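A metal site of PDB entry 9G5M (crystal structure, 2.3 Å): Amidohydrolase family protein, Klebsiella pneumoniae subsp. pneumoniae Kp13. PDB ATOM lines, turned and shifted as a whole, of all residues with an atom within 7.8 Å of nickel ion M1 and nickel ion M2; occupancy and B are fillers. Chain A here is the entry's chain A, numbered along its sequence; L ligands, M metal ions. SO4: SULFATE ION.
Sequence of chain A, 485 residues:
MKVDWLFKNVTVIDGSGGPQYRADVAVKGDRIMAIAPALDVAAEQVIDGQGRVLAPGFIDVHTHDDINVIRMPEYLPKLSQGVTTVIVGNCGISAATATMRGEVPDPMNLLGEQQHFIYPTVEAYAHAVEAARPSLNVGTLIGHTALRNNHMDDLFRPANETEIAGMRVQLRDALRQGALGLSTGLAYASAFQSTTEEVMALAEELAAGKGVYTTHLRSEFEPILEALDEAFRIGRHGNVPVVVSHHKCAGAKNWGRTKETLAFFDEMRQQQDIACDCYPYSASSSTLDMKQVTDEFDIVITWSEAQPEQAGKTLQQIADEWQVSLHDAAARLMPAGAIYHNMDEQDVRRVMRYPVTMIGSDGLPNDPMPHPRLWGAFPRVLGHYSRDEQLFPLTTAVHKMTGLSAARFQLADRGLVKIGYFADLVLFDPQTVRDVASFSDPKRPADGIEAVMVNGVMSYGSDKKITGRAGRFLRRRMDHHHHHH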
ATOM      1  N   HIS A  62      -5.999  33.165  11.170  1.00  0.00           N
ATOM      2  CA  HIS A  62      -6.715  32.215  12.013  1.00  0.00           C
ATOM      3  C   HIS A  62      -6.720  30.830  11.374  1.00  0.00           C
ATOM      4  O   HIS A  62      -7.603  30.506  10.578  1.00  0.00           O
ATOM      5  CB  HIS A  62      -8.120  32.705  12.294  1.00  0.00           C
ATOM      6  CG  HIS A  62      -8.731  32.064  13.490  1.00  0.00           C
ATOM      7  ND1 HIS A  62      -9.212  30.763  13.481  1.00  0.00           N
ATOM      8  CD2 HIS A  62      -8.927  32.524  14.746  1.00  0.00           C
ATOM      9  CE1 HIS A  62      -9.693  30.468  14.676  1.00  0.00           C
ATOM     10  NE2 HIS A  62      -9.536  31.522  15.455  1.00  0.00           N
ATOM     11  N   THR A  63      -5.749  30.009  11.737  1.00  0.00           N
ATOM     12  CA  THR A  63      -5.661  28.661  11.214  1.00  0.00           C
ATOM     13  C   THR A  63      -5.503  27.668  12.357  1.00  0.00           C
ATOM     14  O   THR A  63      -5.115  28.016  13.482  1.00  0.00           O
ATOM     15  CB  THR A  63      -4.478  28.456  10.247  1.00  0.00           C
ATOM     16  OG1 THR A  63      -3.286  28.233  11.002  1.00  0.00           O
ATOM     17  CG2 THR A  63      -4.282  29.690   9.349  1.00  0.00           C
ATOM     18  N   HIS A  64      -5.800  26.420  12.029  1.00  0.00           N
ATOM     19  CA  HIS A  64      -5.476  25.288  12.862  1.00  0.00           C
ATOM     20  C   HIS A  64      -4.589  24.331  12.076  1.00  0.00           C
ATOM     21  O   HIS A  64      -4.799  23.116  12.101  1.00  0.00           O
ATOM     22  CB  HIS A  64      -6.783  24.648  13.349  1.00  0.00           C
ATOM     23  CG  HIS A  64      -7.582  25.559  14.213  1.00  0.00           C
ATOM     24  ND1 HIS A  64      -7.155  25.936  15.475  1.00  0.00           N
ATOM     25  CD2 HIS A  64      -8.740  26.222  13.984  1.00  0.00           C
ATOM     26  CE1 HIS A  64      -8.047  26.771  15.993  1.00  0.00           C
ATOM     27  NE2 HIS A  64      -9.011  26.951  15.117  1.00  0.00           N
ATOM     28  N   GLY A  89      -1.976  27.779  16.015  1.00  0.00           N
ATOM     29  CA  GLY A  89      -2.097  27.802  17.461  1.00  0.00           C
ATOM     30  C   GLY A  89      -3.225  28.636  18.005  1.00  0.00           C
ATOM     31  O   GLY A  89      -3.070  29.274  19.068  1.00  0.00           O
ATOM     32  N   ASN A  90      -4.370  28.663  17.314  1.00  0.00           N
ATOM     33  CA  ASN A  90      -5.491  29.513  17.672  1.00  0.00           C
ATOM     34  C   ASN A  90      -6.473  28.821  18.624  1.00  0.00           C
ATOM     35  O   ASN A  90      -6.375  27.624  18.896  1.00  0.00           O
ATOM     36  CB  ASN A  90      -6.216  29.991  16.414  1.00  0.00           C
ATOM     37  CG  ASN A  90      -5.452  31.076  15.716  1.00  0.00           C
ATOM     38  OD1 ASN A  90      -5.551  32.249  16.061  1.00  0.00           O
ATOM     39  ND2 ASN A  90      -4.635  30.684  14.749  1.00  0.00           N
ATOM     40  N   CYS A  91      -7.417  29.621  19.130  1.00  0.00           N
ATOM     41  CA  CYS A  91      -8.514  29.159  19.996  1.00  0.00           C
ATOM     42  C   CYS A  91      -8.024  28.362  21.200  1.00  0.00           C
ATOM     43  O   CYS A  91      -8.694  27.432  21.662  1.00  0.00           O
ATOM     44  CB  CYS A  91      -9.524  28.353  19.198  1.00  0.00           C
ATOM     45  SG  CYS A  91     -10.157  29.317  17.826  1.00  0.00           S
ATOM     46  N   GLY A  92      -6.871  28.722  21.738  1.00  0.00           N
ATOM     47  CA  GLY A  92      -6.369  28.088  22.933  1.00  0.00           C
ATOM     48  C   GLY A  92      -5.643  26.776  22.723  1.00  0.00           C
ATOM     49  O   GLY A  92      -5.222  26.151  23.711  1.00  0.00           O
ATOM     50  N   ILE A  93      -5.466  26.326  21.473  1.00  0.00           N
ATOM     51  CA  ILE A  93      -4.885  25.018  21.184  1.00  0.00           C
ATOM     52  C   ILE A  93      -3.732  25.198  20.208  1.00  0.00           C
ATOM     53  O   ILE A  93      -3.909  25.762  19.113  1.00  0.00           O
ATOM     54  CB  ILE A  93      -5.922  24.018  20.624  1.00  0.00           C
ATOM     55  CG1 ILE A  93      -6.654  24.596  19.396  1.00  0.00           C
ATOM     56  CG2 ILE A  93      -6.906  23.627  21.716  1.00  0.00           C
ATOM     57  CD1 ILE A  93      -7.341  23.557  18.551  1.00  0.00           C
ATOM     58  N   PRO A 107     -10.462  20.930  22.586  1.00  0.00           N
ATOM     59  CA  PRO A 107     -10.485  20.476  21.188  1.00  0.00           C
ATOM     60  C   PRO A 107      -9.097  20.314  20.568  1.00  0.00           C
ATOM     61  O   PRO A 107      -8.966  20.514  19.356  1.00  0.00           O
ATOM     62  CB  PRO A 107     -11.240  21.603  20.490  1.00  0.00           C
ATOM     63  CG  PRO A 107     -10.717  22.846  21.217  1.00  0.00           C
ATOM     64  CD  PRO A 107     -10.533  22.406  22.673  1.00  0.00           C
ATOM     65  N   LEU A 110      -8.621  18.594  17.211  1.00  0.00           N
ATOM     66  CA  LEU A 110      -8.731  19.216  15.889  1.00  0.00           C
ATOM     67  C   LEU A 110      -7.407  19.193  15.142  1.00  0.00           C
ATOM     68  O   LEU A 110      -7.403  19.171  13.900  1.00  0.00           O
ATOM     69  CB  LEU A 110      -9.211  20.668  16.000  1.00  0.00           C
ATOM     70  CG  LEU A 110     -10.663  20.979  16.401  1.00  0.00           C
ATOM     71  CD1 LEU A 110     -10.912  22.489  16.348  1.00  0.00           C
ATOM     72  CD2 LEU A 110     -11.635  20.266  15.499  1.00  0.00           C
ATOM     73  N   THR A 184      -6.657  32.116  23.351  1.00  0.00           N
ATOM     74  CA  THR A 184      -7.577  31.452  24.269  1.00  0.00           C
ATOM     75  C   THR A 184      -8.771  30.910  23.499  1.00  0.00           C
ATOM     76  O   THR A 184      -9.140  31.416  22.435  1.00  0.00           O
ATOM     77  CB  THR A 184      -8.074  32.374  25.391  1.00  0.00           C
ATOM     78  OG1 THR A 184      -8.740  33.516  24.828  1.00  0.00           O
ATOM     79  CG2 THR A 184      -6.915  32.822  26.276  1.00  0.00           C
ATOM     80  N   GLY A 185      -9.362  29.848  24.053  1.00  0.00           N
ATOM     81  CA  GLY A 185     -10.616  29.306  23.597  1.00  0.00           C
ATOM     82  C   GLY A 185     -11.503  29.059  24.792  1.00  0.00           C
ATOM     83  O   GLY A 185     -11.718  27.904  25.195  1.00  0.00           O
ATOM     84  N   LEU A 186     -12.030  30.144  25.357  1.00  0.00           N
ATOM     85  CA  LEU A 186     -12.642  30.099  26.679  1.00  0.00           C
ATOM     86  C   LEU A 186     -14.030  29.483  26.661  1.00  0.00           C
ATOM     87  O   LEU A 186     -14.538  29.113  27.732  1.00  0.00           O
ATOM     88  CB  LEU A 186     -12.694  31.525  27.242  1.00  0.00           C
ATOM     89  CG  LEU A 186     -11.337  32.210  27.387  1.00  0.00           C
ATOM     90  CD1 LEU A 186     -11.477  33.662  27.850  1.00  0.00           C
ATOM     91  CD2 LEU A 186     -10.426  31.418  28.335  1.00  0.00           C
ATOM     92  N   ALA A 187     -14.668  29.355  25.503  1.00  0.00           N
ATOM     93  CA  ALA A 187     -15.973  28.707  25.452  1.00  0.00           C
ATOM     94  C   ALA A 187     -15.871  27.188  25.571  1.00  0.00           C
ATOM     95  O   ALA A 187     -16.859  26.549  25.919  1.00  0.00           O
ATOM     96  CB  ALA A 187     -16.708  29.059  24.164  1.00  0.00           C
ATOM     97  N   TYR A 188     -14.701  26.612  25.308  1.00  0.00           N
ATOM     98  CA  TYR A 188     -14.548  25.166  25.380  1.00  0.00           C
ATOM     99  C   TYR A 188     -14.487  24.702  26.831  1.00  0.00           C
ATOM    100  O   TYR A 188     -13.896  25.355  27.686  1.00  0.00           O
ATOM    101  CB  TYR A 188     -13.279  24.715  24.629  1.00  0.00           C
ATOM    102  CG  TYR A 188     -13.464  24.834  23.145  1.00  0.00           C
ATOM    103  CD1 TYR A 188     -14.199  23.888  22.434  1.00  0.00           C
ATOM    104  CD2 TYR A 188     -12.921  25.904  22.427  1.00  0.00           C
ATOM    105  CE1 TYR A 188     -14.380  23.994  21.062  1.00  0.00           C
ATOM    106  CE2 TYR A 188     -13.094  26.016  21.054  1.00  0.00           C
ATOM    107  CZ  TYR A 188     -13.830  25.062  20.373  1.00  0.00           C
ATOM    108  OH  TYR A 188     -14.032  25.164  19.006  1.00  0.00           O
ATOM    109  N   THR A 215      -8.370  35.721  21.103  1.00  0.00           N
ATOM    110  CA  THR A 215      -9.335  35.032  21.947  1.00  0.00           C
ATOM    111  C   THR A 215     -10.535  34.557  21.142  1.00  0.00           C
ATOM    112  O   THR A 215     -11.215  35.342  20.468  1.00  0.00           O
ATOM    113  CB  THR A 215      -9.783  35.916  23.105  1.00  0.00           C
ATOM    114  OG1 THR A 215     -10.824  35.230  23.823  1.00  0.00           O
ATOM    115  CG2 THR A 215     -10.295  37.273  22.627  1.00  0.00           C
ATOM    116  N   HIS A 216     -10.779  33.265  21.221  1.00  0.00           N
ATOM    117  CA  HIS A 216     -12.131  32.737  21.068  1.00  0.00           C
ATOM    118  C   HIS A 216     -12.873  33.102  22.344  1.00  0.00           C
ATOM    119  O   HIS A 216     -12.524  32.627  23.426  1.00  0.00           O
ATOM    120  CB  HIS A 216     -12.054  31.240  20.843  1.00  0.00           C
ATOM    121  CG  HIS A 216     -13.376  30.571  20.681  1.00  0.00           C
ATOM    122  ND1 HIS A 216     -13.580  29.553  19.783  1.00  0.00           N
ATOM    123  CD2 HIS A 216     -14.557  30.750  21.324  1.00  0.00           C
ATOM    124  CE1 HIS A 216     -14.834  29.134  19.864  1.00  0.00           C
ATOM    125  NE2 HIS A 216     -15.447  29.848  20.789  1.00  0.00           N
ATOM    126  N   LEU A 217     -13.876  33.972  22.231  1.00  0.00           N
ATOM    127  CA  LEU A 217     -14.578  34.523  23.390  1.00  0.00           C
ATOM    128  C   LEU A 217     -15.193  33.433  24.269  1.00  0.00           C
ATOM    129  O   LEU A 217     -15.561  32.361  23.798  1.00  0.00           O
ATOM    130  CB  LEU A 217     -15.697  35.471  22.951  1.00  0.00           C
ATOM    131  CG  LEU A 217     -15.295  36.742  22.233  1.00  0.00           C
ATOM    132  CD1 LEU A 217     -16.570  37.490  21.845  1.00  0.00           C
ATOM    133  CD2 LEU A 217     -14.371  37.629  23.111  1.00  0.00           C
ATOM    134  N   GLU A 220     -20.018  33.293  22.297  1.00  0.00           N
ATOM    135  CA  GLU A 220     -20.381  34.021  21.076  1.00  0.00           C
ATOM    136  C   GLU A 220     -21.891  34.093  20.891  1.00  0.00           C
ATOM    137  O   GLU A 220     -22.370  34.296  19.766  1.00  0.00           O
ATOM    138  CB  GLU A 220     -19.700  33.384  19.853  1.00  0.00           C
ATOM    139  CG  GLU A 220     -18.183  33.375  19.917  1.00  0.00           C
ATOM    140  CD  GLU A 220     -17.537  33.102  18.559  1.00  0.00           C
ATOM    141  OE1 GLU A 220     -17.853  32.064  17.954  1.00  0.00           O
ATOM    142  OE2 GLU A 220     -16.719  33.938  18.094  1.00  0.00           O
ATOM    143  N   SER A 245     -11.073  36.557  17.867  1.00  0.00           N
ATOM    144  CA  SER A 245     -11.058  35.578  16.795  1.00  0.00           C
ATOM    145  C   SER A 245     -12.456  35.336  16.245  1.00  0.00           C
ATOM    146  O   SER A 245     -13.456  35.411  16.959  1.00  0.00           O
ATOM    147  CB  SER A 245     -10.473  34.244  17.288  1.00  0.00           C
ATOM    148  OG  SER A 245      -9.198  34.425  17.883  1.00  0.00           O
ATOM    149  N   HIS A 246     -12.500  35.001  14.955  1.00  0.00           N
ATOM    150  CA  HIS A 246     -13.726  34.721  14.205  1.00  0.00           C
ATOM    151  C   HIS A 246     -14.945  35.393  14.829  1.00  0.00           C
ATOM    152  O   HIS A 246     -15.923  34.730  15.204  1.00  0.00           O
ATOM    153  CB  HIS A 246     -13.935  33.199  14.058  1.00  0.00           C
ATOM    154  CG  HIS A 246     -13.813  32.419  15.343  1.00  0.00           C
ATOM    155  ND1 HIS A 246     -14.580  32.659  16.449  1.00  0.00           N
ATOM    156  CD2 HIS A 246     -13.022  31.356  15.656  1.00  0.00           C
ATOM    157  CE1 HIS A 246     -14.274  31.796  17.404  1.00  0.00           C
ATOM    158  NE2 HIS A 246     -13.333  30.993  16.949  1.00  0.00           N
ATOM    159  N   LYS A 248     -18.351  36.810  15.503  1.00  0.00           N
ATOM    160  CA  LYS A 248     -19.661  36.503  14.957  1.00  0.00           C
ATOM    161  C   LYS A 248     -20.687  36.670  16.067  1.00  0.00           C
ATOM    162  O   LYS A 248     -20.335  36.661  17.251  1.00  0.00           O
ATOM    163  CB  LYS A 248     -19.730  35.059  14.421  1.00  0.00           C
ATOM    164  CG  LYS A 248     -19.501  34.014  15.522  1.00  0.00           C
ATOM    165  CD  LYS A 248     -19.750  32.592  15.074  1.00  0.00           C
ATOM    166  CE  LYS A 248     -18.614  32.044  14.233  1.00  0.00           C
ATOM    167  NZ  LYS A 248     -17.351  31.972  15.036  1.00  0.00           N
ATOM    168  N   ASP A 277     -10.776  39.232  13.737  1.00  0.00           N
ATOM    169  CA  ASP A 277     -10.842  38.615  12.407  1.00  0.00           C
ATOM    170  C   ASP A 277     -12.181  37.892  12.264  1.00  0.00           C
ATOM    171  O   ASP A 277     -12.917  37.712  13.232  1.00  0.00           O
ATOM    172  CB  ASP A 277      -9.672  37.659  12.151  1.00  0.00           C
ATOM    173  CG  ASP A 277      -9.567  36.544  13.183  1.00  0.00           C
ATOM    174  OD1 ASP A 277     -10.360  35.574  13.124  1.00  0.00           O
ATOM    175  OD2 ASP A 277      -8.695  36.636  14.065  1.00  0.00           O
ATOM    176  N   SER A 361      -9.356  32.235   7.739  1.00  0.00           N
ATOM    177  CA  SER A 361     -10.198  31.183   7.189  1.00  0.00           C
ATOM    178  C   SER A 361     -10.835  30.337   8.280  1.00  0.00           C
ATOM    179  O   SER A 361     -11.954  29.831   8.103  1.00  0.00           O
ATOM    180  CB  SER A 361      -9.399  30.276   6.263  1.00  0.00           C
ATOM    181  OG  SER A 361      -8.477  29.492   7.023  1.00  0.00           O
ATOM    182  N   ASP A 362     -10.149  30.180   9.411  1.00  0.00           N
ATOM    183  CA  ASP A 362     -10.588  29.242  10.436  1.00  0.00           C
ATOM    184  C   ASP A 362     -10.846  27.874   9.809  1.00  0.00           C
ATOM    185  O   ASP A 362     -11.769  27.159  10.196  1.00  0.00           O
ATOM    186  CB  ASP A 362     -11.827  29.753  11.185  1.00  0.00           C
ATOM    187  CG  ASP A 362     -12.061  28.998  12.507  1.00  0.00           C
ATOM    188  OD1 ASP A 362     -11.110  28.366  13.005  1.00  0.00           O
ATOM    189  OD2 ASP A 362     -13.187  29.045  13.032  1.00  0.00           O
ATOM    190  N   GLY A 363     -10.008  27.507   8.850  1.00  0.00           N
ATOM    191  CA  GLY A 363     -10.140  26.206   8.218  1.00  0.00           C
ATOM    192  C   GLY A 363      -9.771  25.076   9.164  1.00  0.00           C
ATOM    193  O   GLY A 363      -8.869  25.180   9.988  1.00  0.00           O
ATOM    194  N   LEU A 364     -10.482  23.961   9.021  1.00  0.00           N
ATOM    195  CA  LEU A 364     -10.265  22.762   9.812  1.00  0.00           C
ATOM    196  C   LEU A 364      -9.788  21.646   8.894  1.00  0.00           C
ATOM    197  O   LEU A 364     -10.608  20.975   8.248  1.00  0.00           O
ATOM    198  CB  LEU A 364     -11.549  22.349  10.551  1.00  0.00           C
ATOM    199  CG  LEU A 364     -12.127  23.430  11.469  1.00  0.00           C
ATOM    200  CD1 LEU A 364     -13.269  22.890  12.318  1.00  0.00           C
ATOM    201  CD2 LEU A 364     -11.054  24.027  12.367  1.00  0.00           C
ATOM    202  N   ARG A 373     -14.495  27.358   3.676  1.00  0.00           N
ATOM    203  CA  ARG A 373     -13.568  28.421   4.031  1.00  0.00           C
ATOM    204  C   ARG A 373     -12.130  27.919   4.030  1.00  0.00           C
ATOM    205  O   ARG A 373     -11.194  28.694   3.831  1.00  0.00           O
ATOM    206  CB  ARG A 373     -13.933  28.995   5.400  1.00  0.00           C
ATOM    207  CG  ARG A 373     -13.809  27.978   6.539  1.00  0.00           C
ATOM    208  CD  ARG A 373     -14.561  28.461   7.767  1.00  0.00           C
ATOM    209  NE  ARG A 373     -14.196  27.691   8.963  1.00  0.00           N
ATOM    210  CZ  ARG A 373     -15.024  27.495   9.983  1.00  0.00           C
ATOM    211  NH1 ARG A 373     -16.271  27.960   9.975  1.00  0.00           N
ATOM    212  NH2 ARG A 373     -14.598  26.815  11.048  1.00  0.00           N
HETATM  213  S   SO4 L   1     -12.703  26.695  16.434  1.00  0.00           S
HETATM  214  O1  SO4 L   1     -13.686  25.765  15.753  1.00  0.00           O
HETATM  215  O2  SO4 L   1     -11.661  25.895  17.153  1.00  0.00           O
HETATM  216  O3  SO4 L   1     -12.131  27.585  15.383  1.00  0.00           O
HETATM  217  O4  SO4 L   1     -13.385  27.507  17.467  1.00  0.00           O
HETATM  218 NI    NI M   1     -12.460  29.287  17.969  1.00  0.00          NI
HETATM  219 NI    NI M   2     -10.144  28.569  15.494  1.00  0.00          NI
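Three residues have an atom within 4 Å of nickel ion M1: Cys 91, His 216 and His 246.
Nickel ion M1 is bound by an oxygen (O4) of the ligand (2.1 Å), a ring nitrogen (ND1) of His 216 (2.1 Å), a ring nitrogen (NE2) of His 246 (2.2 Å) and the side-chain sulfur (SG) of Cys 91 (2.3 Å).
Nickel ion M1 has four donor atoms within binding distance.
A ring nitrogen (NE2) of His 64 is bound to nickel ion M2, 2.0 Å away.
O3 of the ligand binds nickel ion M2.
SG of Cys 91 binds nickel ion M2 (2.4 Å).
Nickel ion M2 has three donor atoms within binding distance.
Slightly farther from nickel ion M2 lies the side-chain carboxylate (OD1) of Asp 362 (2.7 Å).
The side-chain amino group (NZ) of Lys 248 is in hydrogen-bond range of the backbone carbonyl oxygen (O) of His 246, at 3.1 Å.
NH2 of Arg 373 is in salt-bridge range of OD2 of Asp 362 (3.3 Å).
The backbone NH (N) of Asp 362 sits at hydrogen-bond distance from the backbone carbonyl oxygen (O) of His 62, at 2.8 Å.
O of Cys 91 sits close to N of Gly 185, 3.5 Å away.
O of Thr 184 lies within hydrogen-bond range of N of His 216, at 2.8 Å.
A ring nitrogen (ND1) of His 246 is in hydrogen-bond range of the side-chain carboxylate (OE2) of Glu 220.
The backbone carbonyl oxygen (O) of His 216 is in hydrogen-bond range of the backbone NH (N) of Leu 186 (3.2 Å).
N of His 246 is in hydrogen-bond range of OD1 of Asp 277, at 2.9 Å.
Merely in contact with nickel ion M2: His 62 (2.1 Å).
Of the 28 residues printed, 4 come within 4 Å of nickel ion M2.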
